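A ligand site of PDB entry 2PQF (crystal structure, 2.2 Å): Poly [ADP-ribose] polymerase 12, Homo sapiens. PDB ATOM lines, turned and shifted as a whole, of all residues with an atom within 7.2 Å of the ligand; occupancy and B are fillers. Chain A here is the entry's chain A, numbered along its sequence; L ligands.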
ATOM      1  N   PHE A  77      12.656   2.179  -4.624  1.00  0.00           N
ATOM      2  CA  PHE A  77      14.021   1.727  -5.072  1.00  0.00           C
ATOM      3  C   PHE A  77      15.112   2.724  -4.761  1.00  0.00           C
ATOM      4  O   PHE A  77      14.890   3.908  -4.704  1.00  0.00           O
ATOM      5  CB  PHE A  77      14.035   1.373  -6.559  1.00  0.00           C
ATOM      6  CG  PHE A  77      13.248   0.150  -6.872  1.00  0.00           C
ATOM      7  CD1 PHE A  77      13.775  -1.096  -6.654  1.00  0.00           C
ATOM      8  CD2 PHE A  77      11.921   0.258  -7.292  1.00  0.00           C
ATOM      9  CE1 PHE A  77      13.043  -2.205  -6.909  1.00  0.00           C
ATOM     10  CE2 PHE A  77      11.188  -0.861  -7.583  1.00  0.00           C
ATOM     11  CZ  PHE A  77      11.712  -2.076  -7.360  1.00  0.00           C
ATOM     12  N   HIS A  78      16.294   2.191  -4.500  1.00  0.00           N
ATOM     13  CA  HIS A  78      17.496   3.029  -4.370  1.00  0.00           C
ATOM     14  C   HIS A  78      18.751   2.430  -5.059  1.00  0.00           C
ATOM     15  O   HIS A  78      19.390   1.523  -4.549  1.00  0.00           O
ATOM     16  CB  HIS A  78      17.809   3.276  -2.914  1.00  0.00           C
ATOM     17  CG  HIS A  78      18.945   4.215  -2.685  1.00  0.00           C
ATOM     18  ND1 HIS A  78      18.761   5.556  -2.460  1.00  0.00           N
ATOM     19  CD2 HIS A  78      20.288   3.992  -2.597  1.00  0.00           C
ATOM     20  CE1 HIS A  78      19.923   6.128  -2.220  1.00  0.00           C
ATOM     21  NE2 HIS A  78      20.870   5.203  -2.319  1.00  0.00           N
ATOM     22  N   GLY A  79      19.118   3.027  -6.190  1.00  0.00           N
ATOM     23  CA  GLY A  79      20.349   2.664  -6.914  1.00  0.00           C
ATOM     24  C   GLY A  79      21.592   3.196  -6.252  1.00  0.00           C
ATOM     25  O   GLY A  79      21.709   4.393  -5.960  1.00  0.00           O
ATOM     26  N   THR A  80      22.551   2.302  -6.009  1.00  0.00           N
ATOM     27  CA  THR A  80      23.847   2.654  -5.409  1.00  0.00           C
ATOM     28  C   THR A  80      24.922   1.718  -5.986  1.00  0.00           C
ATOM     29  O   THR A  80      24.584   0.722  -6.620  1.00  0.00           O
ATOM     30  CB  THR A  80      23.818   2.536  -3.894  1.00  0.00           C
ATOM     31  OG1 THR A  80      24.918   3.240  -3.304  1.00  0.00           O
ATOM     32  CG2 THR A  80      23.804   1.055  -3.476  1.00  0.00           C
ATOM     33  N   THR A 103      20.451  18.832  -9.057  1.00  0.00           N
ATOM     34  CA  THR A 103      18.992  18.941  -8.984  1.00  0.00           C
ATOM     35  C   THR A 103      18.504  18.282  -7.696  1.00  0.00           C
ATOM     36  O   THR A 103      18.304  17.058  -7.614  1.00  0.00           O
ATOM     37  CB  THR A 103      18.276  18.340 -10.222  1.00  0.00           C
ATOM     38  OG1 THR A 103      18.540  16.937 -10.277  1.00  0.00           O
ATOM     39  CG2 THR A 103      18.772  19.028 -11.524  1.00  0.00           C
ATOM     40  N   TYR A 105      15.713  17.965  -4.523  1.00  0.00           N
ATOM     41  CA  TYR A 105      14.424  18.175  -3.906  1.00  0.00           C
ATOM     42  C   TYR A 105      14.668  18.240  -2.385  1.00  0.00           C
ATOM     43  O   TYR A 105      13.710  18.191  -1.576  1.00  0.00           O
ATOM     44  CB  TYR A 105      13.444  17.051  -4.276  1.00  0.00           C
ATOM     45  CG  TYR A 105      12.874  17.205  -5.663  1.00  0.00           C
ATOM     46  CD1 TYR A 105      13.264  16.355  -6.708  1.00  0.00           C
ATOM     47  CD2 TYR A 105      11.957  18.194  -5.936  1.00  0.00           C
ATOM     48  CE1 TYR A 105      12.735  16.524  -8.000  1.00  0.00           C
ATOM     49  CE2 TYR A 105      11.441  18.362  -7.189  1.00  0.00           C
ATOM     50  CZ  TYR A 105      11.831  17.532  -8.221  1.00  0.00           C
ATOM     51  OH  TYR A 105      11.277  17.725  -9.446  1.00  0.00           O
ATOM     52  N   SER A 109      18.182  11.443   1.589  1.00  0.00           N
ATOM     53  CA  SER A 109      18.284  10.261   0.749  1.00  0.00           C
ATOM     54  C   SER A 109      17.116  10.151  -0.223  1.00  0.00           C
ATOM     55  O   SER A 109      15.993  10.507   0.155  1.00  0.00           O
ATOM     56  CB  SER A 109      18.358   9.013   1.632  1.00  0.00           C
ATOM     57  OG  SER A 109      19.533   9.021   2.400  1.00  0.00           O
ATOM     58  N   TYR A 110      17.377   9.621  -1.444  1.00  0.00           N
ATOM     59  CA  TYR A 110      16.424   9.620  -2.571  1.00  0.00           C
ATOM     60  C   TYR A 110      15.921   8.246  -2.878  1.00  0.00           C
ATOM     61  O   TYR A 110      16.648   7.273  -2.730  1.00  0.00           O
ATOM     62  CB  TYR A 110      17.001  10.226  -3.861  1.00  0.00           C
ATOM     63  CG  TYR A 110      17.055  11.734  -3.824  1.00  0.00           C
ATOM     64  CD1 TYR A 110      17.846  12.374  -2.883  1.00  0.00           C
ATOM     65  CD2 TYR A 110      16.273  12.529  -4.669  1.00  0.00           C
ATOM     66  CE1 TYR A 110      17.881  13.754  -2.773  1.00  0.00           C
ATOM     67  CE2 TYR A 110      16.317  13.948  -4.574  1.00  0.00           C
ATOM     68  CZ  TYR A 110      17.138  14.522  -3.610  1.00  0.00           C
ATOM     69  OH  TYR A 110      17.248  15.862  -3.397  1.00  0.00           O
ATOM     70  N   PHE A 111      14.648   8.144  -3.243  1.00  0.00           N
ATOM     71  CA  PHE A 111      14.038   6.836  -3.524  1.00  0.00           C
ATOM     72  C   PHE A 111      13.106   7.014  -4.660  1.00  0.00           C
ATOM     73  O   PHE A 111      12.566   8.061  -4.816  1.00  0.00           O
ATOM     74  CB  PHE A 111      13.328   6.269  -2.263  1.00  0.00           C
ATOM     75  CG  PHE A 111      14.241   6.175  -1.083  1.00  0.00           C
ATOM     76  CD1 PHE A 111      14.378   7.231  -0.218  1.00  0.00           C
ATOM     77  CD2 PHE A 111      14.966   5.031  -0.865  1.00  0.00           C
ATOM     78  CE1 PHE A 111      15.237   7.165   0.856  1.00  0.00           C
ATOM     79  CE2 PHE A 111      15.842   4.962   0.198  1.00  0.00           C
ATOM     80  CZ  PHE A 111      15.979   6.019   1.063  1.00  0.00           C
ATOM     81  N   ALA A 112      12.973   5.987  -5.489  1.00  0.00           N
ATOM     82  CA  ALA A 112      12.206   6.080  -6.704  1.00  0.00           C
ATOM     83  C   ALA A 112      11.093   5.089  -6.630  1.00  0.00           C
ATOM     84  O   ALA A 112      11.285   3.994  -6.169  1.00  0.00           O
ATOM     85  CB  ALA A 112      13.099   5.772  -7.969  1.00  0.00           C
ATOM     86  N   ARG A 113       9.927   5.487  -7.128  1.00  0.00           N
ATOM     87  CA  ARG A 113       8.853   4.538  -7.387  1.00  0.00           C
ATOM     88  C   ARG A 113       9.239   3.406  -8.358  1.00  0.00           C
ATOM     89  O   ARG A 113       8.988   2.221  -8.108  1.00  0.00           O
ATOM     90  CB  ARG A 113       7.692   5.318  -7.963  1.00  0.00           C
ATOM     91  CG  ARG A 113       6.400   4.514  -8.091  1.00  0.00           C
ATOM     92  CD  ARG A 113       5.288   5.357  -8.717  1.00  0.00           C
ATOM     93  NE  ARG A 113       5.616   5.655 -10.112  1.00  0.00           N
ATOM     94  CZ  ARG A 113       5.023   6.554 -10.880  1.00  0.00           C
ATOM     95  NH1 ARG A 113       3.996   7.270 -10.437  1.00  0.00           N
ATOM     96  NH2 ARG A 113       5.443   6.718 -12.143  1.00  0.00           N
ATOM     97  N   ASP A 114       9.817   3.801  -9.489  1.00  0.00           N
ATOM     98  CA  ASP A 114      10.212   2.889 -10.567  1.00  0.00           C
ATOM     99  C   ASP A 114      11.685   2.515 -10.505  1.00  0.00           C
ATOM    100  O   ASP A 114      12.540   3.393 -10.505  1.00  0.00           O
ATOM    101  CB  ASP A 114       9.979   3.612 -11.883  1.00  0.00           C
ATOM    102  CG  ASP A 114       8.564   4.087 -12.045  1.00  0.00           C
ATOM    103  OD1 ASP A 114       7.650   3.495 -11.432  1.00  0.00           O
ATOM    104  OD2 ASP A 114       8.384   5.058 -12.788  1.00  0.00           O
ATOM    105  N   ALA A 115      11.953   1.204 -10.446  1.00  0.00           N
ATOM    106  CA  ALA A 115      13.292   0.606 -10.627  1.00  0.00           C
ATOM    107  C   ALA A 115      14.031   1.220 -11.783  1.00  0.00           C
ATOM    108  O   ALA A 115      15.198   1.548 -11.664  1.00  0.00           O
ATOM    109  CB  ALA A 115      13.176  -0.914 -10.864  1.00  0.00           C
ATOM    110  N   TYR A 117      14.030   4.194 -12.922  1.00  0.00           N
ATOM    111  CA  TYR A 117      14.673   5.488 -12.569  1.00  0.00           C
ATOM    112  C   TYR A 117      15.962   5.317 -11.735  1.00  0.00           C
ATOM    113  O   TYR A 117      16.903   6.080 -11.873  1.00  0.00           O
ATOM    114  CB  TYR A 117      13.689   6.452 -11.845  1.00  0.00           C
ATOM    115  CG  TYR A 117      14.159   7.911 -11.771  1.00  0.00           C
ATOM    116  CD1 TYR A 117      13.894   8.801 -12.789  1.00  0.00           C
ATOM    117  CD2 TYR A 117      14.887   8.378 -10.685  1.00  0.00           C
ATOM    118  CE1 TYR A 117      14.343  10.131 -12.737  1.00  0.00           C
ATOM    119  CE2 TYR A 117      15.340   9.697 -10.625  1.00  0.00           C
ATOM    120  CZ  TYR A 117      15.049  10.562 -11.640  1.00  0.00           C
ATOM    121  OH  TYR A 117      15.500  11.851 -11.557  1.00  0.00           O
ATOM    122  N   SER A 118      15.961   4.323 -10.841  1.00  0.00           N
ATOM    123  CA  SER A 118      17.109   4.011 -10.024  1.00  0.00           C
ATOM    124  C   SER A 118      18.321   3.357 -10.785  1.00  0.00           C
ATOM    125  O   SER A 118      19.476   3.405 -10.312  1.00  0.00           O
ATOM    126  CB  SER A 118      16.640   3.095  -8.867  1.00  0.00           C
ATOM    127  OG  SER A 118      15.853   3.810  -7.934  1.00  0.00           O
ATOM    128  N   HIS A 119      18.048   2.702 -11.908  1.00  0.00           N
ATOM    129  CA  HIS A 119      19.102   2.191 -12.794  1.00  0.00           C
ATOM    130  C   HIS A 119      20.244   3.188 -12.970  1.00  0.00           C
ATOM    131  O   HIS A 119      21.401   2.872 -12.650  1.00  0.00           O
ATOM    132  CB  HIS A 119      18.546   1.798 -14.165  1.00  0.00           C
ATOM    133  CG  HIS A 119      19.575   1.190 -15.066  1.00  0.00           C
ATOM    134  ND1 HIS A 119      20.366   0.129 -14.657  1.00  0.00           N
ATOM    135  CD2 HIS A 119      19.956   1.491 -16.328  1.00  0.00           C
ATOM    136  CE1 HIS A 119      21.184  -0.197 -15.647  1.00  0.00           C
ATOM    137  NE2 HIS A 119      20.973   0.616 -16.659  1.00  0.00           N
ATOM    138  N   HIS A 120      19.929   4.403 -13.389  1.00  0.00           N
ATOM    139  CA  HIS A 120      20.959   5.415 -13.575  1.00  0.00           C
ATOM    140  C   HIS A 120      21.890   5.622 -12.380  1.00  0.00           C
ATOM    141  O   HIS A 120      23.036   5.981 -12.591  1.00  0.00           O
ATOM    142  CB  HIS A 120      20.357   6.762 -13.999  1.00  0.00           C
ATOM    143  CG  HIS A 120      21.392   7.824 -14.243  1.00  0.00           C
ATOM    144  ND1 HIS A 120      21.765   8.736 -13.282  1.00  0.00           N
ATOM    145  CD2 HIS A 120      22.169   8.079 -15.336  1.00  0.00           C
ATOM    146  CE1 HIS A 120      22.709   9.526 -13.767  1.00  0.00           C
ATOM    147  NE2 HIS A 120      22.967   9.148 -15.008  1.00  0.00           N
ATOM    148  N   TYR A 121      21.442   5.380 -11.142  1.00  0.00           N
ATOM    149  CA  TYR A 121      22.268   5.572  -9.939  1.00  0.00           C
ATOM    150  C   TYR A 121      22.975   4.301  -9.482  1.00  0.00           C
ATOM    151  O   TYR A 121      23.739   4.348  -8.503  1.00  0.00           O
ATOM    152  CB  TYR A 121      21.393   6.119  -8.773  1.00  0.00           C
ATOM    153  CG  TYR A 121      20.798   7.455  -9.130  1.00  0.00           C
ATOM    154  CD1 TYR A 121      19.600   7.543  -9.791  1.00  0.00           C
ATOM    155  CD2 TYR A 121      21.492   8.630  -8.856  1.00  0.00           C
ATOM    156  CE1 TYR A 121      19.089   8.766 -10.177  1.00  0.00           C
ATOM    157  CE2 TYR A 121      21.005   9.860  -9.246  1.00  0.00           C
ATOM    158  CZ  TYR A 121      19.795   9.929  -9.900  1.00  0.00           C
ATOM    159  OH  TYR A 121      19.272  11.164 -10.254  1.00  0.00           O
ATOM    160  N   SER A 122      22.673   3.179 -10.125  1.00  0.00           N
ATOM    161  CA  SER A 122      23.357   1.909  -9.903  1.00  0.00           C
ATOM    162  C   SER A 122      24.660   1.828 -10.746  1.00  0.00           C
ATOM    163  O   SER A 122      24.711   1.147 -11.795  1.00  0.00           O
ATOM    164  CB  SER A 122      22.445   0.735 -10.251  1.00  0.00           C
ATOM    165  OG  SER A 122      21.366   0.624  -9.320  1.00  0.00           O
ATOM    166  N   MET A 131      20.958  -2.567  -6.907  1.00  0.00           N
ATOM    167  CA  MET A 131      19.852  -1.697  -6.435  1.00  0.00           C
ATOM    168  C   MET A 131      19.174  -2.269  -5.159  1.00  0.00           C
ATOM    169  O   MET A 131      18.986  -3.473  -5.011  1.00  0.00           O
ATOM    170  CB  MET A 131      18.806  -1.685  -7.523  1.00  0.00           C
ATOM    171  CG  MET A 131      17.900  -0.564  -7.554  1.00  0.00           C
ATOM    172  SD  MET A 131      16.508  -0.998  -8.828  1.00  0.00           S
ATOM    173  CE  MET A 131      17.534  -0.479 -10.478  1.00  0.00           C
ATOM    174  N   PHE A 132      18.840  -1.387  -4.219  1.00  0.00           N
ATOM    175  CA  PHE A 132      18.055  -1.772  -3.037  1.00  0.00           C
ATOM    176  C   PHE A 132      16.551  -1.627  -3.315  1.00  0.00           C
ATOM    177  O   PHE A 132      16.157  -0.706  -4.006  1.00  0.00           O
ATOM    178  CB  PHE A 132      18.428  -0.868  -1.837  1.00  0.00           C
ATOM    179  CG  PHE A 132      19.639  -1.311  -1.061  1.00  0.00           C
ATOM    180  CD1 PHE A 132      19.512  -2.135   0.026  1.00  0.00           C
ATOM    181  CD2 PHE A 132      20.927  -0.872  -1.405  1.00  0.00           C
ATOM    182  CE1 PHE A 132      20.593  -2.528   0.760  1.00  0.00           C
ATOM    183  CE2 PHE A 132      22.054  -1.293  -0.704  1.00  0.00           C
ATOM    184  CZ  PHE A 132      21.896  -2.102   0.405  1.00  0.00           C
ATOM    185  N   SER A 173       6.930  10.329  -7.879  1.00  0.00           N
ATOM    186  CA  SER A 173       7.803   9.221  -8.303  1.00  0.00           C
ATOM    187  C   SER A 173       9.196   9.296  -7.731  1.00  0.00           C
ATOM    188  O   SER A 173       9.916   8.333  -7.817  1.00  0.00           O
ATOM    189  CB  SER A 173       7.829   9.086  -9.839  1.00  0.00           C
ATOM    190  OG  SER A 173       8.355  10.239 -10.451  1.00  0.00           O
ATOM    191  N   ILE A 174       9.534  10.413  -7.124  1.00  0.00           N
ATOM    192  CA  ILE A 174      10.772  10.583  -6.407  1.00  0.00           C
ATOM    193  C   ILE A 174      10.447  11.103  -4.990  1.00  0.00           C
ATOM    194  O   ILE A 174       9.734  12.095  -4.846  1.00  0.00           O
ATOM    195  CB  ILE A 174      11.699  11.607  -7.134  1.00  0.00           C
ATOM    196  CG1 ILE A 174      12.142  11.050  -8.512  1.00  0.00           C
ATOM    197  CG2 ILE A 174      12.860  11.960  -6.208  1.00  0.00           C
ATOM    198  CD1 ILE A 174      12.990  12.034  -9.348  1.00  0.00           C
ATOM    199  N   PHE A 175      10.968  10.418  -3.977  1.00  0.00           N
ATOM    200  CA  PHE A 175      10.831  10.809  -2.575  1.00  0.00           C
ATOM    201  C   PHE A 175      12.186  11.083  -1.924  1.00  0.00           C
ATOM    202  O   PHE A 175      13.145  10.338  -2.134  1.00  0.00           O
ATOM    203  CB  PHE A 175      10.149   9.690  -1.823  1.00  0.00           C
ATOM    204  CG  PHE A 175       8.811   9.283  -2.400  1.00  0.00           C
ATOM    205  CD1 PHE A 175       7.612   9.742  -1.832  1.00  0.00           C
ATOM    206  CD2 PHE A 175       8.741   8.427  -3.482  1.00  0.00           C
ATOM    207  CE1 PHE A 175       6.381   9.340  -2.359  1.00  0.00           C
ATOM    208  CE2 PHE A 175       7.533   8.043  -3.998  1.00  0.00           C
ATOM    209  CZ  PHE A 175       6.343   8.510  -3.435  1.00  0.00           C
HETATM  210  C1  LIG L   1      18.439   6.478  -6.415  1.00  0.00           C
HETATM  211  O1  LIG L   1      19.508   6.631  -5.805  1.00  0.00           O
HETATM  212  O2  LIG L   1      17.930   5.407  -6.800  1.00  0.00           O
HETATM  213  C2  LIG L   1      17.738   7.739  -6.698  1.00  0.00           C
HETATM  214  C3  LIG L   1      16.390   7.690  -6.879  1.00  0.00           C
HETATM  215  C4  LIG L   1      15.728   8.864  -7.135  1.00  0.00           C
HETATM  216  C5  LIG L   1      16.372  10.074  -7.256  1.00  0.00           C
HETATM  217  C6  LIG L   1      17.748  10.130  -7.070  1.00  0.00           C
HETATM  218  C7  LIG L   1      18.427   8.943  -6.766  1.00  0.00           C
HETATM  219  N1  LIG L   1      14.442   8.755  -7.337  1.00  0.00           N
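The side-chain hydroxyl (OG) of Ser 118 lies within hydrogen-bond range of an oxygen (O2) of the ligand. The backbone carbonyl oxygen (O) of Phe 111 is in hydrogen-bond range of a nitrogen (N1) of the ligand (3.2 Å). O2 of the ligand sits at hydrogen-bond distance from N of Gly 79, 2.7 Å away.
N of His 78 sits at hydrogen-bond distance from O of Phe 132 (2.9 Å). O of Phe 175 sits at hydrogen-bond distance from N of Phe 111 (2.9 Å). O of Ala 112 sits at hydrogen-bond distance from N of Phe 77 (2.7 Å). O of Tyr 121 lies within hydrogen-bond range of N of Thr 80, at 3.4 Å. The backbone carbonyl oxygen (O) of Tyr 110 lies within hydrogen-bond range of a ring nitrogen (ND1) of His 78, at 2.7 Å. O of Phe 77 sits close to OG of Ser 118, at 3.4 Å. N of Tyr 105 lies within hydrogen-bond range of OH of Tyr 110 (2.8 Å).
O of Phe 77 touches O2 of the ligand (3.99 Å). His 78 touches the ligand (CA to O2, 3.4 Å). Tyr 110 touches the ligand (CB to C6, 3.3 Å). CB of Ala 112 touches N1 of the ligand, at 3.3 Å. CD2 of Tyr 117 touches N1 of the ligand, 3.4 Å away. Tyr 121 touches the ligand (CE1 to C7, 3.5 Å). Ile 174 touches the ligand (CG1 to N1, 3.5 Å). Hydrophobic or aromatic side chains that line the ligand: His 78, Tyr 110, Ala 112, Tyr 117, Tyr 121 and Ile 174. Of the 24 residues printed, 10 come within 4 Å of the ligand. The nearest printed residue that does not touch the ligand is Ser 173 (4.6 Å).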
